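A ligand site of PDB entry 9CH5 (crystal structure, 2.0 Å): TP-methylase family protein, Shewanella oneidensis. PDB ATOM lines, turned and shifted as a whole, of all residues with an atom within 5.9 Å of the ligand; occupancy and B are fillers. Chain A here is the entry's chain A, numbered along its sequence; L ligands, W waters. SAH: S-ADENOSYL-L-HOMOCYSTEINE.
O of Phe 99 lies close to SD of the ligand, 3.0 Å away. A nitrogen (N3) of the ligand sits close to the backbone carbonyl oxygen (O) of Ile 234, at 2.9 Å. Merely in contact with the ligand: Leu 11 (3.3 Å), Gly 94 (3.5 Å), Ser 124 (3.1 Å), Trp 166 (3.3 Å), Tyr 206 (3.6 Å) and Glu 207 (3.5 Å). Hydrophobic or aromatic side chains that line the ligand: Leu 11, Tyr 93, His 95, Phe 99, Ala 125, Trp 166, Tyr 206, Ala 208 and Ile 234. The nearest printed residue that does not touch the ligand is Asn 210 (4.2 Å).
Water W3 lies within hydrogen-bond range of a nitrogen (N) of the ligand and the backbone carbonyl oxygen of Tyr 93. Water W1 bridges ND2 of Asn 210 and N6 of the ligand.
The side-chain hydroxyl of Ser 124 lies close to the backbone NH of Glu 126 (3.4 Å). N of Gly 97 sits at hydrogen-bond distance from ND1 of His 95 (3.0 Å). OG of Ser 235 lies within hydrogen-bond range of N of Met 232, at 3.0 Å. The side-chain hydroxyl of Ser 235 sits at hydrogen-bond distance from the side-chain carboxylate of Glu 207 (2.5 Å). O of Thr 236 sits at hydrogen-bond distance from N of Tyr 206. The side-chain amide nitrogen (ND2) of Asn 210 lies within hydrogen-bond range of the backbone carbonyl oxygen (O) of Leu 11 (3.0 Å).
N of Gln 167 sits at hydrogen-bond distance from O2' of the ligand. The backbone carbonyl oxygen (O) of Ser 235 is in hydrogen-bond range of an oxygen (O2') of the ligand, at 3.3 Å. The backbone carbonyl oxygen of Val 98 sits at hydrogen-bond distance from a nitrogen (N) of the ligand, 2.9 Å away. O of Ala 208 lies within hydrogen-bond range of N6 of the ligand (3.2 Å). N of Ala 125 sits at hydrogen-bond distance from O of the ligand (3.0 Å). The backbone NH (N) of His 95 is in hydrogen-bond range of an oxygen (OXT) of the ligand (2.9 Å). The backbone carbonyl oxygen (O) of His 95 lies within hydrogen-bond range of a nitrogen (N) of the ligand (3.0 Å). OE1 of Gln 167 lies close to SD of the ligand (3.7 Å). N of Ala 208 lies within hydrogen-bond range of N1 of the ligand (2.8 Å). The backbone carbonyl oxygen of Tyr 93 lies within hydrogen-bond range of a nitrogen (N) of the ligand, 3.5 Å away. An oxygen (O3') of the ligand sits at hydrogen-bond distance from the backbone carbonyl oxygen (O) of Pro 233, at 2.8 Å. An oxygen (O2') of the ligand is in hydrogen-bond range of the side-chain hydroxyl (OG1) of Thr 236.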
ATOM      1  N   LEU A  11       0.355  10.850 -27.522  1.00  0.00           N
ATOM      2  CA  LEU A  11      -0.386  10.767 -28.769  1.00  0.00           C
ATOM      3  C   LEU A  11       0.517  10.933 -29.977  1.00  0.00           C
ATOM      4  O   LEU A  11       0.307  10.272 -31.009  1.00  0.00           O
ATOM      5  CB  LEU A  11      -1.495  11.825 -28.807  1.00  0.00           C
ATOM      6  CG  LEU A  11      -2.816  11.516 -28.077  1.00  0.00           C
ATOM      7  CD1 LEU A  11      -3.599  10.447 -28.807  1.00  0.00           C
ATOM      8  CD2 LEU A  11      -2.611  11.132 -26.618  1.00  0.00           C
ATOM      9  N   TYR A  93      -0.938   3.930 -25.619  1.00  0.00           N
ATOM     10  CA  TYR A  93      -0.836   5.276 -26.170  1.00  0.00           C
ATOM     11  C   TYR A  93      -1.512   6.271 -25.239  1.00  0.00           C
ATOM     12  O   TYR A  93      -2.486   5.964 -24.554  1.00  0.00           O
ATOM     13  CB  TYR A  93      -1.439   5.336 -27.581  1.00  0.00           C
ATOM     14  CG  TYR A  93      -2.953   5.346 -27.672  1.00  0.00           C
ATOM     15  CD1 TYR A  93      -3.668   6.535 -27.567  1.00  0.00           C
ATOM     16  CD2 TYR A  93      -3.652   4.170 -27.886  1.00  0.00           C
ATOM     17  CE1 TYR A  93      -5.047   6.538 -27.657  1.00  0.00           C
ATOM     18  CE2 TYR A  93      -5.034   4.167 -27.983  1.00  0.00           C
ATOM     19  CZ  TYR A  93      -5.724   5.364 -27.869  1.00  0.00           C
ATOM     20  OH  TYR A  93      -7.102   5.368 -27.960  1.00  0.00           O
ATOM     21  N   GLY A  94      -0.967   7.488 -25.222  1.00  0.00           N
ATOM     22  CA  GLY A  94      -1.502   8.530 -24.351  1.00  0.00           C
ATOM     23  C   GLY A  94      -1.105   8.302 -22.916  1.00  0.00           C
ATOM     24  O   GLY A  94       0.063   8.030 -22.607  1.00  0.00           O
ATOM     25  N   HIS A  95      -2.071   8.419 -22.008  1.00  0.00           N
ATOM     26  CA  HIS A  95      -1.930   8.137 -20.580  1.00  0.00           C
ATOM     27  C   HIS A  95      -2.553   6.777 -20.292  1.00  0.00           C
ATOM     28  O   HIS A  95      -3.725   6.566 -20.626  1.00  0.00           O
ATOM     29  CB  HIS A  95      -2.619   9.231 -19.765  1.00  0.00           C
ATOM     30  CG  HIS A  95      -2.497   9.079 -18.270  1.00  0.00           C
ATOM     31  ND1 HIS A  95      -2.706   7.893 -17.611  1.00  0.00           N
ATOM     32  CD2 HIS A  95      -2.218   9.999 -17.317  1.00  0.00           C
ATOM     33  CE1 HIS A  95      -2.554   8.075 -16.309  1.00  0.00           C
ATOM     34  NE2 HIS A  95      -2.261   9.345 -16.102  1.00  0.00           N
ATOM     35  N   PRO A  96      -1.828   5.845 -19.682  1.00  0.00           N
ATOM     36  CA  PRO A  96      -2.299   4.449 -19.652  1.00  0.00           C
ATOM     37  C   PRO A  96      -3.516   4.230 -18.768  1.00  0.00           C
ATOM     38  O   PRO A  96      -4.178   3.192 -18.907  1.00  0.00           O
ATOM     39  CB  PRO A  96      -1.079   3.679 -19.120  1.00  0.00           C
ATOM     40  CG  PRO A  96      -0.395   4.678 -18.247  1.00  0.00           C
ATOM     41  CD  PRO A  96      -0.535   5.981 -18.984  1.00  0.00           C
ATOM     42  N   GLY A  97      -3.830   5.157 -17.858  1.00  0.00           N
ATOM     43  CA  GLY A  97      -4.963   4.999 -16.980  1.00  0.00           C
ATOM     44  C   GLY A  97      -6.095   5.977 -17.229  1.00  0.00           C
ATOM     45  O   GLY A  97      -6.972   6.143 -16.376  1.00  0.00           O
ATOM     46  N   VAL A  98      -6.075   6.631 -18.379  1.00  0.00           N
ATOM     47  CA  VAL A  98      -7.089   7.613 -18.739  1.00  0.00           C
ATOM     48  C   VAL A  98      -7.995   6.986 -19.792  1.00  0.00           C
ATOM     49  O   VAL A  98      -7.554   6.730 -20.927  1.00  0.00           O
ATOM     50  CB  VAL A  98      -6.470   8.932 -19.236  1.00  0.00           C
ATOM     51  CG1 VAL A  98      -7.527   9.801 -19.894  1.00  0.00           C
ATOM     52  CG2 VAL A  98      -5.819   9.671 -18.080  1.00  0.00           C
ATOM     53  N   PHE A  99      -9.244   6.753 -19.417  1.00  0.00           N
ATOM     54  CA  PHE A  99     -10.220   6.052 -20.255  1.00  0.00           C
ATOM     55  C   PHE A  99      -9.618   4.786 -20.849  1.00  0.00           C
ATOM     56  O   PHE A  99      -9.725   4.522 -22.049  1.00  0.00           O
ATOM     57  CB  PHE A  99     -10.767   6.975 -21.348  1.00  0.00           C
ATOM     58  CG  PHE A  99     -11.723   8.018 -20.839  1.00  0.00           C
ATOM     59  CD1 PHE A  99     -11.259   9.154 -20.200  1.00  0.00           C
ATOM     60  CD2 PHE A  99     -13.090   7.850 -20.998  1.00  0.00           C
ATOM     61  CE1 PHE A  99     -12.138  10.112 -19.737  1.00  0.00           C
ATOM     62  CE2 PHE A  99     -13.979   8.809 -20.532  1.00  0.00           C
ATOM     63  CZ  PHE A  99     -13.496   9.942 -19.899  1.00  0.00           C
ATOM     64  N   ALA A 100      -8.978   3.992 -19.999  1.00  0.00           N
ATOM     65  CA  ALA A 100      -8.374   2.734 -20.408  1.00  0.00           C
ATOM     66  C   ALA A 100      -8.356   1.814 -19.207  1.00  0.00           C
ATOM     67  O   ALA A 100      -7.836   2.175 -18.147  1.00  0.00           O
ATOM     68  CB  ALA A 100      -6.967   2.947 -20.960  1.00  0.00           C
ATOM     69  N   ILE A 123       0.892  11.637 -21.234  1.00  0.00           N
ATOM     70  CA  ILE A 123       0.177  12.761 -21.830  1.00  0.00           C
ATOM     71  C   ILE A 123      -1.010  12.218 -22.623  1.00  0.00           C
ATOM     72  O   ILE A 123      -0.826  11.506 -23.610  1.00  0.00           O
ATOM     73  CB  ILE A 123       1.098  13.603 -22.726  1.00  0.00           C
ATOM     74  CG1 ILE A 123       2.234  14.197 -21.884  1.00  0.00           C
ATOM     75  CG2 ILE A 123       0.320  14.692 -23.442  1.00  0.00           C
ATOM     76  CD1 ILE A 123       3.417  14.680 -22.696  1.00  0.00           C
ATOM     77  N   SER A 124      -2.218  12.567 -22.197  1.00  0.00           N
ATOM     78  CA  SER A 124      -3.446  12.007 -22.753  1.00  0.00           C
ATOM     79  C   SER A 124      -4.005  12.918 -23.844  1.00  0.00           C
ATOM     80  O   SER A 124      -3.493  14.004 -24.116  1.00  0.00           O
ATOM     81  CB  SER A 124      -4.474  11.781 -21.646  1.00  0.00           C
ATOM     82  OG  SER A 124      -5.007  13.014 -21.192  1.00  0.00           O
ATOM     83  N   ALA A 125      -5.082  12.449 -24.487  1.00  0.00           N
ATOM     84  CA  ALA A 125      -5.729  13.251 -25.517  1.00  0.00           C
ATOM     85  C   ALA A 125      -6.348  14.507 -24.935  1.00  0.00           C
ATOM     86  O   ALA A 125      -6.393  15.545 -25.606  1.00  0.00           O
ATOM     87  CB  ALA A 125      -6.792  12.414 -26.233  1.00  0.00           C
ATOM     88  N   GLU A 126      -6.819  14.434 -23.681  1.00  0.00           N
ATOM     89  CA  GLU A 126      -7.330  15.616 -23.004  1.00  0.00           C
ATOM     90  C   GLU A 126      -6.237  16.661 -22.843  1.00  0.00           C
ATOM     91  O   GLU A 126      -6.464  17.857 -23.071  1.00  0.00           O
ATOM     92  CB  GLU A 126      -7.906  15.232 -21.652  1.00  0.00           C
ATOM     93  CG  GLU A 126      -8.396  16.382 -20.808  1.00  0.00           C
ATOM     94  CD  GLU A 126      -8.316  16.088 -19.328  1.00  0.00           C
ATOM     95  OE1 GLU A 126      -9.122  15.260 -18.851  1.00  0.00           O
ATOM     96  OE2 GLU A 126      -7.449  16.672 -18.646  1.00  0.00           O
ATOM     97  N   LEU A 165     -17.065  14.574 -24.186  1.00  0.00           N
ATOM     98  CA  LEU A 165     -17.652  13.244 -24.310  1.00  0.00           C
ATOM     99  C   LEU A 165     -16.665  12.374 -25.084  1.00  0.00           C
ATOM    100  O   LEU A 165     -16.464  12.566 -26.290  1.00  0.00           O
ATOM    101  CB  LEU A 165     -19.014  13.289 -25.002  1.00  0.00           C
ATOM    102  CG  LEU A 165     -20.099  14.088 -24.263  1.00  0.00           C
ATOM    103  CD1 LEU A 165     -21.444  13.918 -24.937  1.00  0.00           C
ATOM    104  CD2 LEU A 165     -20.169  13.689 -22.794  1.00  0.00           C
ATOM    105  N   TRP A 166     -16.049  11.423 -24.396  1.00  0.00           N
ATOM    106  CA  TRP A 166     -15.058  10.547 -25.004  1.00  0.00           C
ATOM    107  C   TRP A 166     -15.751   9.393 -25.732  1.00  0.00           C
ATOM    108  O   TRP A 166     -16.885   9.024 -25.418  1.00  0.00           O
ATOM    109  CB  TRP A 166     -14.097   9.974 -23.958  1.00  0.00           C
ATOM    110  CG  TRP A 166     -13.269  11.005 -23.230  1.00  0.00           C
ATOM    111  CD1 TRP A 166     -13.712  12.100 -22.552  1.00  0.00           C
ATOM    112  CD2 TRP A 166     -11.839  11.003 -23.108  1.00  0.00           C
ATOM    113  NE1 TRP A 166     -12.645  12.789 -22.019  1.00  0.00           N
ATOM    114  CE2 TRP A 166     -11.490  12.140 -22.352  1.00  0.00           C
ATOM    115  CE3 TRP A 166     -10.823  10.161 -23.578  1.00  0.00           C
ATOM    116  CZ2 TRP A 166     -10.159  12.442 -22.040  1.00  0.00           C
ATOM    117  CZ3 TRP A 166      -9.511  10.475 -23.267  1.00  0.00           C
ATOM    118  CH2 TRP A 166      -9.193  11.604 -22.503  1.00  0.00           C
ATOM    119  N   GLN A 167     -15.024   8.824 -26.694  1.00  0.00           N
ATOM    120  CA  GLN A 167     -15.520   7.691 -27.486  1.00  0.00           C
ATOM    121  C   GLN A 167     -16.873   8.012 -28.108  1.00  0.00           C
ATOM    122  O   GLN A 167     -17.801   7.194 -28.106  1.00  0.00           O
ATOM    123  CB  GLN A 167     -15.574   6.422 -26.635  1.00  0.00           C
ATOM    124  CG  GLN A 167     -14.306   6.192 -25.817  1.00  0.00           C
ATOM    125  CD  GLN A 167     -14.209   4.787 -25.237  1.00  0.00           C
ATOM    126  OE1 GLN A 167     -13.131   4.205 -25.180  1.00  0.00           O
ATOM    127  NE2 GLN A 167     -15.340   4.249 -24.799  1.00  0.00           N
ATOM    128  N   ILE A 168     -16.978   9.221 -28.660  1.00  0.00           N
ATOM    129  CA  ILE A 168     -18.229   9.690 -29.246  1.00  0.00           C
ATOM    130  C   ILE A 168     -18.638   8.830 -30.437  1.00  0.00           C
ATOM    131  O   ILE A 168     -19.827   8.715 -30.747  1.00  0.00           O
ATOM    132  CB  ILE A 168     -18.085  11.182 -29.635  1.00  0.00           C
ATOM    133  CG1 ILE A 168     -19.415  11.751 -30.157  1.00  0.00           C
ATOM    134  CG2 ILE A 168     -16.965  11.375 -30.659  1.00  0.00           C
ATOM    135  CD1 ILE A 168     -20.476  11.861 -29.094  1.00  0.00           C
ATOM    136  N   TYR A 206     -12.679  17.050 -32.016  1.00  0.00           N
ATOM    137  CA  TYR A 206     -11.235  17.188 -31.865  1.00  0.00           C
ATOM    138  C   TYR A 206     -10.558  15.849 -32.076  1.00  0.00           C
ATOM    139  O   TYR A 206     -11.010  14.820 -31.561  1.00  0.00           O
ATOM    140  CB  TYR A 206     -10.881  17.742 -30.479  1.00  0.00           C
ATOM    141  CG  TYR A 206      -9.399  17.729 -30.166  1.00  0.00           C
ATOM    142  CD1 TYR A 206      -8.532  18.605 -30.793  1.00  0.00           C
ATOM    143  CD2 TYR A 206      -8.873  16.829 -29.235  1.00  0.00           C
ATOM    144  CE1 TYR A 206      -7.184  18.602 -30.511  1.00  0.00           C
ATOM    145  CE2 TYR A 206      -7.524  16.818 -28.946  1.00  0.00           C
ATOM    146  CZ  TYR A 206      -6.689  17.702 -29.579  1.00  0.00           C
ATOM    147  OH  TYR A 206      -5.340  17.698 -29.297  1.00  0.00           O
ATOM    148  N   GLU A 207      -9.467  15.856 -32.852  1.00  0.00           N
ATOM    149  CA  GLU A 207      -8.588  14.698 -32.959  1.00  0.00           C
ATOM    150  C   GLU A 207      -7.149  15.197 -32.885  1.00  0.00           C
ATOM    151  O   GLU A 207      -6.675  15.882 -33.796  1.00  0.00           O
ATOM    152  CB  GLU A 207      -8.830  13.918 -34.249  1.00  0.00           C
ATOM    153  CG  GLU A 207     -10.216  13.285 -34.346  1.00  0.00           C
ATOM    154  CD  GLU A 207     -10.506  12.725 -35.728  1.00  0.00           C
ATOM    155  OE1 GLU A 207      -9.577  12.691 -36.563  1.00  0.00           O
ATOM    156  OE2 GLU A 207     -11.659  12.307 -35.968  1.00  0.00           O
ATOM    157  N   ALA A 208      -6.464  14.875 -31.787  1.00  0.00           N
ATOM    158  CA  ALA A 208      -5.043  15.165 -31.669  1.00  0.00           C
ATOM    159  C   ALA A 208      -4.265  14.420 -32.742  1.00  0.00           C
ATOM    160  O   ALA A 208      -4.612  13.298 -33.129  1.00  0.00           O
ATOM    161  CB  ALA A 208      -4.533  14.765 -30.278  1.00  0.00           C
ATOM    162  N   ALA A 209      -3.207  15.043 -33.231  1.00  0.00           N
ATOM    163  CA  ALA A 209      -2.402  14.449 -34.276  1.00  0.00           C
ATOM    164  C   ALA A 209      -1.527  13.329 -33.714  1.00  0.00           C
ATOM    165  O   ALA A 209      -1.044  13.404 -32.592  1.00  0.00           O
ATOM    166  CB  ALA A 209      -1.527  15.502 -34.956  1.00  0.00           C
ATOM    167  N   ASN A 210      -1.344  12.285 -34.523  1.00  0.00           N
ATOM    168  CA  ASN A 210      -0.461  11.178 -34.167  1.00  0.00           C
ATOM    169  C   ASN A 210       0.900  11.271 -34.833  1.00  0.00           C
ATOM    170  O   ASN A 210       1.834  10.591 -34.399  1.00  0.00           O
ATOM    171  CB  ASN A 210      -1.107   9.835 -34.528  1.00  0.00           C
ATOM    172  CG  ASN A 210      -2.356   9.547 -33.710  1.00  0.00           C
ATOM    173  OD1 ASN A 210      -3.433   9.340 -34.267  1.00  0.00           O
ATOM    174  ND2 ASN A 210      -2.216   9.535 -32.393  1.00  0.00           N
ATOM    175  N   MET A 232     -14.540   9.162 -36.018  1.00  0.00           N
ATOM    176  CA  MET A 232     -13.561   8.096 -35.984  1.00  0.00           C
ATOM    177  C   MET A 232     -13.381   7.625 -34.553  1.00  0.00           C
ATOM    178  O   MET A 232     -13.747   8.335 -33.607  1.00  0.00           O
ATOM    179  CB  MET A 232     -12.217   8.578 -36.566  1.00  0.00           C
ATOM    180  CG  MET A 232     -12.283   8.969 -38.022  1.00  0.00           C
ATOM    181  SD  MET A 232     -12.645   7.575 -39.096  1.00  0.00           S
ATOM    182  CE  MET A 232     -11.143   6.619 -38.933  1.00  0.00           C
ATOM    183  N   PRO A 233     -12.832   6.427 -34.344  1.00  0.00           N
ATOM    184  CA  PRO A 233     -12.540   5.972 -32.976  1.00  0.00           C
ATOM    185  C   PRO A 233     -11.689   6.934 -32.160  1.00  0.00           C
ATOM    186  O   PRO A 233     -11.811   6.947 -30.926  1.00  0.00           O
ATOM    187  CB  PRO A 233     -11.813   4.646 -33.205  1.00  0.00           C
ATOM    188  CG  PRO A 233     -12.402   4.134 -34.481  1.00  0.00           C
ATOM    189  CD  PRO A 233     -12.581   5.352 -35.336  1.00  0.00           C
ATOM    190  N   ILE A 234     -10.843   7.757 -32.788  1.00  0.00           N
ATOM    191  CA  ILE A 234     -10.000   8.682 -32.048  1.00  0.00           C
ATOM    192  C   ILE A 234     -10.667  10.024 -31.803  1.00  0.00           C
ATOM    193  O   ILE A 234     -10.031  10.935 -31.261  1.00  0.00           O
ATOM    194  CB  ILE A 234      -8.636   8.893 -32.743  1.00  0.00           C
ATOM    195  CG1 ILE A 234      -8.832   9.361 -34.193  1.00  0.00           C
ATOM    196  CG2 ILE A 234      -7.792   7.635 -32.684  1.00  0.00           C
ATOM    197  CD1 ILE A 234      -7.638  10.092 -34.762  1.00  0.00           C
ATOM    198  N   SER A 235     -11.932  10.177 -32.190  1.00  0.00           N
ATOM    199  CA  SER A 235     -12.623  11.453 -32.058  1.00  0.00           C
ATOM    200  C   SER A 235     -13.104  11.666 -30.624  1.00  0.00           C
ATOM    201  O   SER A 235     -13.638  10.754 -29.993  1.00  0.00           O
ATOM    202  CB  SER A 235     -13.803  11.530 -33.023  1.00  0.00           C
ATOM    203  OG  SER A 235     -13.379  11.438 -34.367  1.00  0.00           O
ATOM    204  N   THR A 236     -12.908  12.884 -30.127  1.00  0.00           N
ATOM    205  CA  THR A 236     -13.499  13.352 -28.881  1.00  0.00           C
ATOM    206  C   THR A 236     -14.376  14.554 -29.167  1.00  0.00           C
ATOM    207  O   THR A 236     -13.974  15.452 -29.920  1.00  0.00           O
ATOM    208  CB  THR A 236     -12.420  13.698 -27.850  1.00  0.00           C
ATOM    209  OG1 THR A 236     -11.663  12.534 -27.528  1.00  0.00           O
ATOM    210  CG2 THR A 236     -13.041  14.250 -26.579  1.00  0.00           C
HETATM  211  N   SAH L   1      -5.575   6.413 -23.007  1.00  0.00           N
HETATM  212  CA  SAH L   1      -6.010   7.289 -24.084  1.00  0.00           C
HETATM  213  CB  SAH L   1      -7.518   7.145 -24.270  1.00  0.00           C
HETATM  214  CG  SAH L   1      -7.959   5.788 -24.832  1.00  0.00           C
HETATM  215  SD  SAH L   1      -9.754   5.602 -24.883  1.00  0.00           S
HETATM  216  C   SAH L   1      -5.618   8.738 -23.835  1.00  0.00           C
HETATM  217  O   SAH L   1      -6.203   9.665 -24.395  1.00  0.00           O
HETATM  218  OXT SAH L   1      -4.702   9.000 -23.060  1.00  0.00           O
HETATM  219  C5' SAH L   1     -10.112   6.095 -26.581  1.00  0.00           C
HETATM  220  C4' SAH L   1     -10.739   7.476 -26.592  1.00  0.00           C
HETATM  221  O4' SAH L   1      -9.773   8.439 -26.225  1.00  0.00           O
HETATM  222  C3' SAH L   1     -11.236   7.873 -27.973  1.00  0.00           C
HETATM  223  O3' SAH L   1     -12.540   7.401 -28.225  1.00  0.00           O
HETATM  224  C2' SAH L   1     -11.200   9.372 -27.854  1.00  0.00           C
HETATM  225  O2' SAH L   1     -12.310   9.829 -27.122  1.00  0.00           O
HETATM  226  C1' SAH L   1      -9.943   9.579 -27.034  1.00  0.00           C
HETATM  227  N9  SAH L   1      -8.820   9.706 -27.965  1.00  0.00           N
HETATM  228  C8  SAH L   1      -7.935   8.713 -28.347  1.00  0.00           C
HETATM  229  N7  SAH L   1      -7.078   9.243 -29.259  1.00  0.00           N
HETATM  230  C5  SAH L   1      -7.436  10.517 -29.479  1.00  0.00           C
HETATM  231  C6  SAH L   1      -6.911  11.504 -30.305  1.00  0.00           C
HETATM  232  N6  SAH L   1      -5.859  11.251 -31.082  1.00  0.00           N
HETATM  233  N1  SAH L   1      -7.491  12.752 -30.323  1.00  0.00           N
HETATM  234  C2  SAH L   1      -8.574  13.032 -29.526  1.00  0.00           C
HETATM  235  N3  SAH L   1      -9.090  12.052 -28.709  1.00  0.00           N
HETATM  236  C4  SAH L   1      -8.535  10.823 -28.682  1.00  0.00           C
HETATM  237  O   HOH W   1      -4.487   8.594 -31.269  1.00  0.00           O
HETATM  238  O   HOH W   2     -14.696   8.349 -30.788  1.00  0.00           O
HETATM  239  O   HOH W   3      -4.685   4.032 -23.960  1.00  0.00           O
